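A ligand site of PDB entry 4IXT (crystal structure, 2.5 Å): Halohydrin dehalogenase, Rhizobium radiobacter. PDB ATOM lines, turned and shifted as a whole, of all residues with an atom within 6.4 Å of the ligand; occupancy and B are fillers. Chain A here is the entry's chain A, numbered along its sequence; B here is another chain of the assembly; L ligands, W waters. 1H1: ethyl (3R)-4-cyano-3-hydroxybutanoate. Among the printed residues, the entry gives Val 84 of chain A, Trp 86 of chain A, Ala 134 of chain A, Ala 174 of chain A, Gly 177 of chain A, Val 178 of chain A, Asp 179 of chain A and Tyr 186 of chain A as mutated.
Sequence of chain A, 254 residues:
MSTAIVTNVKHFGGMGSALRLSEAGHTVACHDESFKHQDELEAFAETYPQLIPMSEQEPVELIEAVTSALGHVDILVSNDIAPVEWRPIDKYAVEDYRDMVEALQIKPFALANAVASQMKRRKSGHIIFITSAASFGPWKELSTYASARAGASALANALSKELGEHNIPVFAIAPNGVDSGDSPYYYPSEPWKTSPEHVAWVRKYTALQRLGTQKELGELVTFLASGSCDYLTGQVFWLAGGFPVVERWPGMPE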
ATOM      1  N   PHE A  12      24.400  27.605  22.053  1.00  0.00           N
ATOM      2  CA  PHE A  12      23.529  26.417  21.935  1.00  0.00           C
ATOM      3  C   PHE A  12      23.484  25.980  20.456  1.00  0.00           C
ATOM      4  O   PHE A  12      24.511  25.560  19.918  1.00  0.00           O
ATOM      5  CB  PHE A  12      22.131  26.722  22.532  1.00  0.00           C
ATOM      6  CG  PHE A  12      21.302  25.503  22.843  1.00  0.00           C
ATOM      7  CD1 PHE A  12      21.846  24.226  22.822  1.00  0.00           C
ATOM      8  CD2 PHE A  12      19.959  25.640  23.186  1.00  0.00           C
ATOM      9  CE1 PHE A  12      21.061  23.116  23.159  1.00  0.00           C
ATOM     10  CE2 PHE A  12      19.166  24.536  23.493  1.00  0.00           C
ATOM     11  CZ  PHE A  12      19.715  23.278  23.469  1.00  0.00           C
ATOM     12  N   VAL A  84      21.459  26.137  33.754  1.00  0.00           N
ATOM     13  CA  VAL A  84      20.891  25.075  34.562  1.00  0.00           C
ATOM     14  C   VAL A  84      21.411  25.191  35.986  1.00  0.00           C
ATOM     15  O   VAL A  84      22.601  25.468  36.210  1.00  0.00           O
ATOM     16  CB  VAL A  84      21.232  23.665  34.030  1.00  0.00           C
ATOM     17  CG1 VAL A  84      21.006  23.576  32.533  1.00  0.00           C
ATOM     18  CG2 VAL A  84      22.669  23.299  34.351  1.00  0.00           C
ATOM     19  N   TRP A  86      21.723  23.085  39.356  1.00  0.00           N
ATOM     20  CA  TRP A  86      21.604  21.714  39.870  1.00  0.00           C
ATOM     21  C   TRP A  86      21.258  21.581  41.362  1.00  0.00           C
ATOM     22  O   TRP A  86      21.829  20.741  42.053  1.00  0.00           O
ATOM     23  CB  TRP A  86      22.900  20.933  39.607  1.00  0.00           C
ATOM     24  CG  TRP A  86      23.290  20.738  38.162  1.00  0.00           C
ATOM     25  CD1 TRP A  86      24.034  21.593  37.382  1.00  0.00           C
ATOM     26  CD2 TRP A  86      23.124  19.536  37.386  1.00  0.00           C
ATOM     27  NE1 TRP A  86      24.301  21.012  36.163  1.00  0.00           N
ATOM     28  CE2 TRP A  86      23.748  19.750  36.134  1.00  0.00           C
ATOM     29  CE3 TRP A  86      22.483  18.305  37.615  1.00  0.00           C
ATOM     30  CZ2 TRP A  86      23.744  18.796  35.120  1.00  0.00           C
ATOM     31  CZ3 TRP A  86      22.477  17.363  36.612  1.00  0.00           C
ATOM     32  CH2 TRP A  86      23.106  17.611  35.375  1.00  0.00           C
ATOM     33  N   THR A 131      14.695  22.784  22.249  1.00  0.00           N
ATOM     34  CA  THR A 131      14.421  22.489  23.655  1.00  0.00           C
ATOM     35  C   THR A 131      15.587  21.654  24.233  1.00  0.00           C
ATOM     36  O   THR A 131      16.727  22.116  24.210  1.00  0.00           O
ATOM     37  CB  THR A 131      12.983  21.867  23.862  1.00  0.00           C
ATOM     38  OG1 THR A 131      12.871  20.591  23.212  1.00  0.00           O
ATOM     39  CG2 THR A 131      11.923  22.795  23.308  1.00  0.00           C
ATOM     40  N   SER A 132      15.323  20.442  24.723  1.00  0.00           N
ATOM     41  CA  SER A 132      16.400  19.628  25.345  1.00  0.00           C
ATOM     42  C   SER A 132      15.977  18.165  25.587  1.00  0.00           C
ATOM     43  O   SER A 132      14.862  17.897  26.034  1.00  0.00           O
ATOM     44  CB  SER A 132      16.825  20.257  26.691  1.00  0.00           C
ATOM     45  OG  SER A 132      17.530  19.322  27.501  1.00  0.00           O
ATOM     46  N   ALA A 133      16.903  17.224  25.365  1.00  0.00           N
ATOM     47  CA  ALA A 133      16.625  15.810  25.719  1.00  0.00           C
ATOM     48  C   ALA A 133      16.389  15.598  27.220  1.00  0.00           C
ATOM     49  O   ALA A 133      16.042  14.486  27.635  1.00  0.00           O
ATOM     50  CB  ALA A 133      17.715  14.852  25.198  1.00  0.00           C
ATOM     51  N   ALA A 134      16.580  16.642  28.023  1.00  0.00           N
ATOM     52  CA  ALA A 134      16.295  16.573  29.443  1.00  0.00           C
ATOM     53  C   ALA A 134      14.796  16.383  29.739  1.00  0.00           C
ATOM     54  O   ALA A 134      14.427  15.935  30.830  1.00  0.00           O
ATOM     55  CB  ALA A 134      16.824  17.807  30.151  1.00  0.00           C
ATOM     56  N   TRP A 139      18.343  12.422  34.388  1.00  0.00           N
ATOM     57  CA  TRP A 139      19.082  13.215  35.370  1.00  0.00           C
ATOM     58  C   TRP A 139      18.377  13.383  36.702  1.00  0.00           C
ATOM     59  O   TRP A 139      17.159  13.277  36.774  1.00  0.00           O
ATOM     60  CB  TRP A 139      19.448  14.586  34.803  1.00  0.00           C
ATOM     61  CG  TRP A 139      20.723  14.545  34.056  1.00  0.00           C
ATOM     62  CD1 TRP A 139      21.994  14.375  34.572  1.00  0.00           C
ATOM     63  CD2 TRP A 139      20.874  14.575  32.639  1.00  0.00           C
ATOM     64  NE1 TRP A 139      22.921  14.339  33.561  1.00  0.00           N
ATOM     65  CE2 TRP A 139      22.261  14.471  32.360  1.00  0.00           C
ATOM     66  CE3 TRP A 139      19.979  14.743  31.590  1.00  0.00           C
ATOM     67  CZ2 TRP A 139      22.760  14.542  31.073  1.00  0.00           C
ATOM     68  CZ3 TRP A 139      20.479  14.765  30.318  1.00  0.00           C
ATOM     69  CH2 TRP A 139      21.853  14.660  30.067  1.00  0.00           C
ATOM     70  N   LEU A 142      17.654  18.438  38.391  1.00  0.00           N
ATOM     71  CA  LEU A 142      17.492  19.326  37.247  1.00  0.00           C
ATOM     72  C   LEU A 142      15.984  19.641  37.056  1.00  0.00           C
ATOM     73  O   LEU A 142      15.514  19.824  35.938  1.00  0.00           O
ATOM     74  CB  LEU A 142      17.998  18.585  36.005  1.00  0.00           C
ATOM     75  CG  LEU A 142      18.845  19.377  35.040  1.00  0.00           C
ATOM     76  CD1 LEU A 142      19.877  20.161  35.824  1.00  0.00           C
ATOM     77  CD2 LEU A 142      19.488  18.462  33.998  1.00  0.00           C
ATOM     78  N   TYR A 145      14.540  22.568  35.217  1.00  0.00           N
ATOM     79  CA  TYR A 145      15.025  22.625  33.839  1.00  0.00           C
ATOM     80  C   TYR A 145      14.374  21.573  32.935  1.00  0.00           C
ATOM     81  O   TYR A 145      13.896  21.902  31.849  1.00  0.00           O
ATOM     82  CB  TYR A 145      16.560  22.528  33.783  1.00  0.00           C
ATOM     83  CG  TYR A 145      17.141  22.607  32.378  1.00  0.00           C
ATOM     84  CD1 TYR A 145      17.391  21.461  31.629  1.00  0.00           C
ATOM     85  CD2 TYR A 145      17.419  23.852  31.803  1.00  0.00           C
ATOM     86  CE1 TYR A 145      17.896  21.543  30.349  1.00  0.00           C
ATOM     87  CE2 TYR A 145      17.932  23.940  30.509  1.00  0.00           C
ATOM     88  CZ  TYR A 145      18.157  22.794  29.782  1.00  0.00           C
ATOM     89  OH  TYR A 145      18.685  22.904  28.512  1.00  0.00           O
ATOM     90  N   ARG A 149      11.541  22.575  29.818  1.00  0.00           N
ATOM     91  CA  ARG A 149      11.816  22.066  28.492  1.00  0.00           C
ATOM     92  C   ARG A 149      10.697  21.176  27.967  1.00  0.00           C
ATOM     93  O   ARG A 149      10.383  21.241  26.769  1.00  0.00           O
ATOM     94  CB  ARG A 149      13.191  21.410  28.434  1.00  0.00           C
ATOM     95  CG  ARG A 149      14.359  22.392  28.640  1.00  0.00           C
ATOM     96  CD  ARG A 149      14.621  23.240  27.412  1.00  0.00           C
ATOM     97  NE  ARG A 149      16.012  23.702  27.345  1.00  0.00           N
ATOM     98  CZ  ARG A 149      16.463  24.627  26.488  1.00  0.00           C
ATOM     99  NH1 ARG A 149      15.628  25.208  25.634  1.00  0.00           N
ATOM    100  NH2 ARG A 149      17.741  25.011  26.517  1.00  0.00           N
ATOM    101  N   ALA A 174      15.086  18.344  20.532  1.00  0.00           N
ATOM    102  CA  ALA A 174      15.528  18.093  21.914  1.00  0.00           C
ATOM    103  C   ALA A 174      16.958  17.482  21.938  1.00  0.00           C
ATOM    104  O   ALA A 174      17.114  16.280  21.694  1.00  0.00           O
ATOM    105  CB  ALA A 174      14.527  17.166  22.629  1.00  0.00           C
ATOM    106  N   PRO A 175      17.991  18.329  22.135  1.00  0.00           N
ATOM    107  CA  PRO A 175      19.375  17.874  22.043  1.00  0.00           C
ATOM    108  C   PRO A 175      19.957  17.357  23.376  1.00  0.00           C
ATOM    109  O   PRO A 175      19.476  17.694  24.465  1.00  0.00           O
ATOM    110  CB  PRO A 175      20.123  19.152  21.607  1.00  0.00           C
ATOM    111  CG  PRO A 175      19.085  20.148  21.210  1.00  0.00           C
ATOM    112  CD  PRO A 175      17.893  19.783  22.030  1.00  0.00           C
ATOM    113  N   ASN A 176      20.978  16.519  23.268  1.00  0.00           N
ATOM    114  CA  ASN A 176      21.966  16.359  24.323  1.00  0.00           C
ATOM    115  C   ASN A 176      23.344  16.227  23.728  1.00  0.00           C
ATOM    116  O   ASN A 176      23.521  15.571  22.701  1.00  0.00           O
ATOM    117  CB  ASN A 176      21.688  15.117  25.177  1.00  0.00           C
ATOM    118  CG  ASN A 176      22.667  14.981  26.341  1.00  0.00           C
ATOM    119  OD1 ASN A 176      22.603  15.753  27.301  1.00  0.00           O
ATOM    120  ND2 ASN A 176      23.629  14.040  26.223  1.00  0.00           N
ATOM    121  N   GLY A 177      24.332  16.823  24.407  1.00  0.00           N
ATOM    122  CA  GLY A 177      25.748  16.601  24.097  1.00  0.00           C
ATOM    123  C   GLY A 177      26.176  17.186  22.766  1.00  0.00           C
ATOM    124  O   GLY A 177      27.064  16.628  22.090  1.00  0.00           O
ATOM    125  N   VAL A 178      25.508  18.252  22.349  1.00  0.00           N
ATOM    126  CA  VAL A 178      25.926  18.970  21.148  1.00  0.00           C
ATOM    127  C   VAL A 178      27.020  20.014  21.463  1.00  0.00           C
ATOM    128  O   VAL A 178      26.827  20.935  22.265  1.00  0.00           O
ATOM    129  CB  VAL A 178      24.722  19.648  20.416  1.00  0.00           C
ATOM    130  CG1 VAL A 178      25.221  20.418  19.211  1.00  0.00           C
ATOM    131  CG2 VAL A 178      23.658  18.584  19.985  1.00  0.00           C
ATOM    132  N   ASP A 179      28.187  19.802  20.882  1.00  0.00           N
ATOM    133  CA  ASP A 179      29.332  20.682  21.020  1.00  0.00           C
ATOM    134  C   ASP A 179      28.926  22.125  20.777  1.00  0.00           C
ATOM    135  O   ASP A 179      28.420  22.444  19.714  1.00  0.00           O
ATOM    136  CB  ASP A 179      30.375  20.267  19.991  1.00  0.00           C
ATOM    137  CG  ASP A 179      31.604  21.178  19.965  1.00  0.00           C
ATOM    138  OD1 ASP A 179      31.722  22.153  20.750  1.00  0.00           O
ATOM    139  OD2 ASP A 179      32.514  20.834  19.184  1.00  0.00           O
ATOM    140  N   TYR A 185      26.461  27.069  26.918  1.00  0.00           N
ATOM    141  CA  TYR A 185      25.194  26.323  26.716  1.00  0.00           C
ATOM    142  C   TYR A 185      25.308  25.404  25.503  1.00  0.00           C
ATOM    143  O   TYR A 185      25.249  25.902  24.379  1.00  0.00           O
ATOM    144  CB  TYR A 185      24.049  27.306  26.438  1.00  0.00           C
ATOM    145  CG  TYR A 185      24.009  28.487  27.371  1.00  0.00           C
ATOM    146  CD1 TYR A 185      23.303  28.429  28.564  1.00  0.00           C
ATOM    147  CD2 TYR A 185      24.654  29.690  27.057  1.00  0.00           C
ATOM    148  CE1 TYR A 185      23.238  29.517  29.419  1.00  0.00           C
ATOM    149  CE2 TYR A 185      24.622  30.780  27.910  1.00  0.00           C
ATOM    150  CZ  TYR A 185      23.887  30.683  29.086  1.00  0.00           C
ATOM    151  OH  TYR A 185      23.810  31.747  29.959  1.00  0.00           O
ATOM    152  N   TYR A 186      25.439  24.086  25.700  1.00  0.00           N
ATOM    153  CA  TYR A 186      25.573  23.476  27.043  1.00  0.00           C
ATOM    154  C   TYR A 186      26.792  22.538  27.116  1.00  0.00           C
ATOM    155  O   TYR A 186      27.084  21.955  28.159  1.00  0.00           O
ATOM    156  CB  TYR A 186      24.276  22.721  27.457  1.00  0.00           C
ATOM    157  CG  TYR A 186      23.109  23.646  27.763  1.00  0.00           C
ATOM    158  CD1 TYR A 186      22.934  24.187  29.058  1.00  0.00           C
ATOM    159  CD2 TYR A 186      22.252  24.096  26.747  1.00  0.00           C
ATOM    160  CE1 TYR A 186      21.930  25.123  29.312  1.00  0.00           C
ATOM    161  CE2 TYR A 186      21.264  25.034  26.983  1.00  0.00           C
ATOM    162  CZ  TYR A 186      21.065  25.507  28.273  1.00  0.00           C
ATOM    163  OH  TYR A 186      20.069  26.426  28.503  1.00  0.00           O
ATOM    164  N   TYR A 187      27.465  22.364  25.980  1.00  0.00           N
ATOM    165  CA  TYR A 187      28.680  21.542  25.936  1.00  0.00           C
ATOM    166  C   TYR A 187      29.899  22.230  25.300  1.00  0.00           C
ATOM    167  O   TYR A 187      30.300  21.901  24.198  1.00  0.00           O
ATOM    168  CB  TYR A 187      28.395  20.192  25.274  1.00  0.00           C
ATOM    169  CG  TYR A 187      27.545  19.250  26.115  1.00  0.00           C
ATOM    170  CD1 TYR A 187      26.156  19.385  26.175  1.00  0.00           C
ATOM    171  CD2 TYR A 187      28.134  18.223  26.838  1.00  0.00           C
ATOM    172  CE1 TYR A 187      25.385  18.539  26.965  1.00  0.00           C
ATOM    173  CE2 TYR A 187      27.388  17.374  27.640  1.00  0.00           C
ATOM    174  CZ  TYR A 187      26.017  17.525  27.703  1.00  0.00           C
ATOM    175  OH  TYR A 187      25.271  16.661  28.485  1.00  0.00           O
ATOM    176  N   LEU A 239      17.858  14.369  19.721  1.00  0.00           N
ATOM    177  CA  LEU A 239      19.081  14.642  19.007  1.00  0.00           C
ATOM    178  C   LEU A 239      20.199  14.396  20.009  1.00  0.00           C
ATOM    179  O   LEU A 239      20.852  15.346  20.450  1.00  0.00           O
ATOM    180  CB  LEU A 239      19.093  16.091  18.591  1.00  0.00           C
ATOM    181  CG  LEU A 239      19.916  16.558  17.388  1.00  0.00           C
ATOM    182  CD1 LEU A 239      20.839  17.684  17.739  1.00  0.00           C
ATOM    183  CD2 LEU A 239      20.644  15.439  16.646  1.00  0.00           C
ATOM    184  N   PHE A 243      22.076   8.627  23.823  1.00  0.00           N
ATOM    185  CA  PHE A 243      22.093   8.844  25.270  1.00  0.00           C
ATOM    186  C   PHE A 243      20.711   8.602  25.881  1.00  0.00           C
ATOM    187  O   PHE A 243      19.692   8.977  25.291  1.00  0.00           O
ATOM    188  CB  PHE A 243      22.574  10.272  25.568  1.00  0.00           C
ATOM    189  CG  PHE A 243      22.506  10.628  27.023  1.00  0.00           C
ATOM    190  CD1 PHE A 243      21.403  11.283  27.536  1.00  0.00           C
ATOM    191  CD2 PHE A 243      23.547  10.300  27.881  1.00  0.00           C
ATOM    192  CE1 PHE A 243      21.327  11.598  28.880  1.00  0.00           C
ATOM    193  CE2 PHE A 243      23.467  10.588  29.240  1.00  0.00           C
ATOM    194  CZ  PHE A 243      22.359  11.250  29.732  1.00  0.00           C
ATOM    195  N   TRP B 249      27.253  15.435  35.451  1.00  0.00           N
ATOM    196  CA  TRP B 249      28.567  15.792  34.854  1.00  0.00           C
ATOM    197  C   TRP B 249      29.774  15.703  35.807  1.00  0.00           C
ATOM    198  O   TRP B 249      29.741  16.284  36.904  1.00  0.00           O
ATOM    199  CB  TRP B 249      28.527  17.222  34.277  1.00  0.00           C
ATOM    200  CG  TRP B 249      27.498  17.492  33.195  1.00  0.00           C
ATOM    201  CD1 TRP B 249      27.018  16.595  32.284  1.00  0.00           C
ATOM    202  CD2 TRP B 249      26.934  18.765  32.847  1.00  0.00           C
ATOM    203  NE1 TRP B 249      26.151  17.233  31.415  1.00  0.00           N
ATOM    204  CE2 TRP B 249      26.093  18.560  31.728  1.00  0.00           C
ATOM    205  CE3 TRP B 249      27.035  20.054  33.392  1.00  0.00           C
ATOM    206  CZ2 TRP B 249      25.367  19.596  31.142  1.00  0.00           C
ATOM    207  CZ3 TRP B 249      26.303  21.080  32.798  1.00  0.00           C
ATOM    208  CH2 TRP B 249      25.477  20.841  31.688  1.00  0.00           C
HETATM  209  O2  1H1 L   1      20.310  17.546  29.174  1.00  0.00           O
HETATM  210  C3  1H1 L   1      21.093  18.376  28.747  1.00  0.00           C
HETATM  211  O1  1H1 L   1      21.955  19.077  29.691  1.00  0.00           O
HETATM  212  C2  1H1 L   1      22.323  18.403  30.907  1.00  0.00           C
HETATM  213  C1  1H1 L   1      21.600  19.055  32.058  1.00  0.00           C
HETATM  214  C4  1H1 L   1      21.182  18.660  27.264  1.00  0.00           C
HETATM  215  C5  1H1 L   1      21.135  20.166  27.005  1.00  0.00           C
HETATM  216  O3  1H1 L   1      19.988  20.726  27.673  1.00  0.00           O
HETATM  217  C6  1H1 L   1      21.014  20.438  25.507  1.00  0.00           C
HETATM  218  C7  1H1 L   1      22.253  20.054  24.786  1.00  0.00           C
HETATM  219  N   1H1 L   1      23.194  19.798  24.168  1.00  0.00           N
HETATM  220  O   HOH W   1      24.843  22.149  23.569  1.00  0.00           O
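Residues that only touch the ligand: Leu 142 (2.9 Å), Trp 139 (3.0 Å), Trp 249 of chain B (3.3 Å), Pro 175 (3.3 Å), Phe 12 (3.6 Å), Tyr 187 (3.6 Å), Ala 134 (3.6 Å) and Trp 86 (3.7 Å).
Along chain A the residues within 4 Å of the ligand span positions 12 to 187.
The nearest printed residue that does not touch the ligand is Tyr 186 (4.1 Å).
Water W1 lies within hydrogen-bond range of O of Val 178, N of the ligand and N of Tyr 186.
The backbone NH (N) of Ala 134 sits at hydrogen-bond distance from the side-chain hydroxyl (OG) of Ser 132 (2.9 Å).
The side-chain hydroxyl (OH) of Tyr 145 sits at hydrogen-bond distance from the guanidinium group (NE) of Arg 149, 3.0 Å away.
The backbone NH (N) of Phe 12 lies within hydrogen-bond range of the backbone carbonyl oxygen (O) of Tyr 185.
OD1 of Asn 176 sits at hydrogen-bond distance from OH of Tyr 187 (3.1 Å).
OH of Tyr 187 is in hydrogen-bond range of NE1 of Trp 249 of chain B (3.1 Å).
N of Asn 176 sits at hydrogen-bond distance from O of Leu 239, 3.1 Å away.
The backbone carbonyl oxygen (O) of Pro 175 sits at hydrogen-bond distance from the backbone NH (N) of Ala 133.
An oxygen (O3) of the ligand sits at hydrogen-bond distance from the side-chain hydroxyl (OH) of Tyr 145.
A nitrogen (N) of the ligand sits at hydrogen-bond distance from the backbone NH (N) of Gly 177 (3.2 Å).
An oxygen (O3) of the ligand lies within hydrogen-bond range of the side-chain hydroxyl (OG) of Ser 132 (2.8 Å).
An oxygen (O2) of the ligand sits close to the side-chain amide oxygen (OD1) of Asn 176 (3.5 Å).
A nitrogen (N) of the ligand lies within hydrogen-bond range of the backbone NH of Val 178 (3.3 Å).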
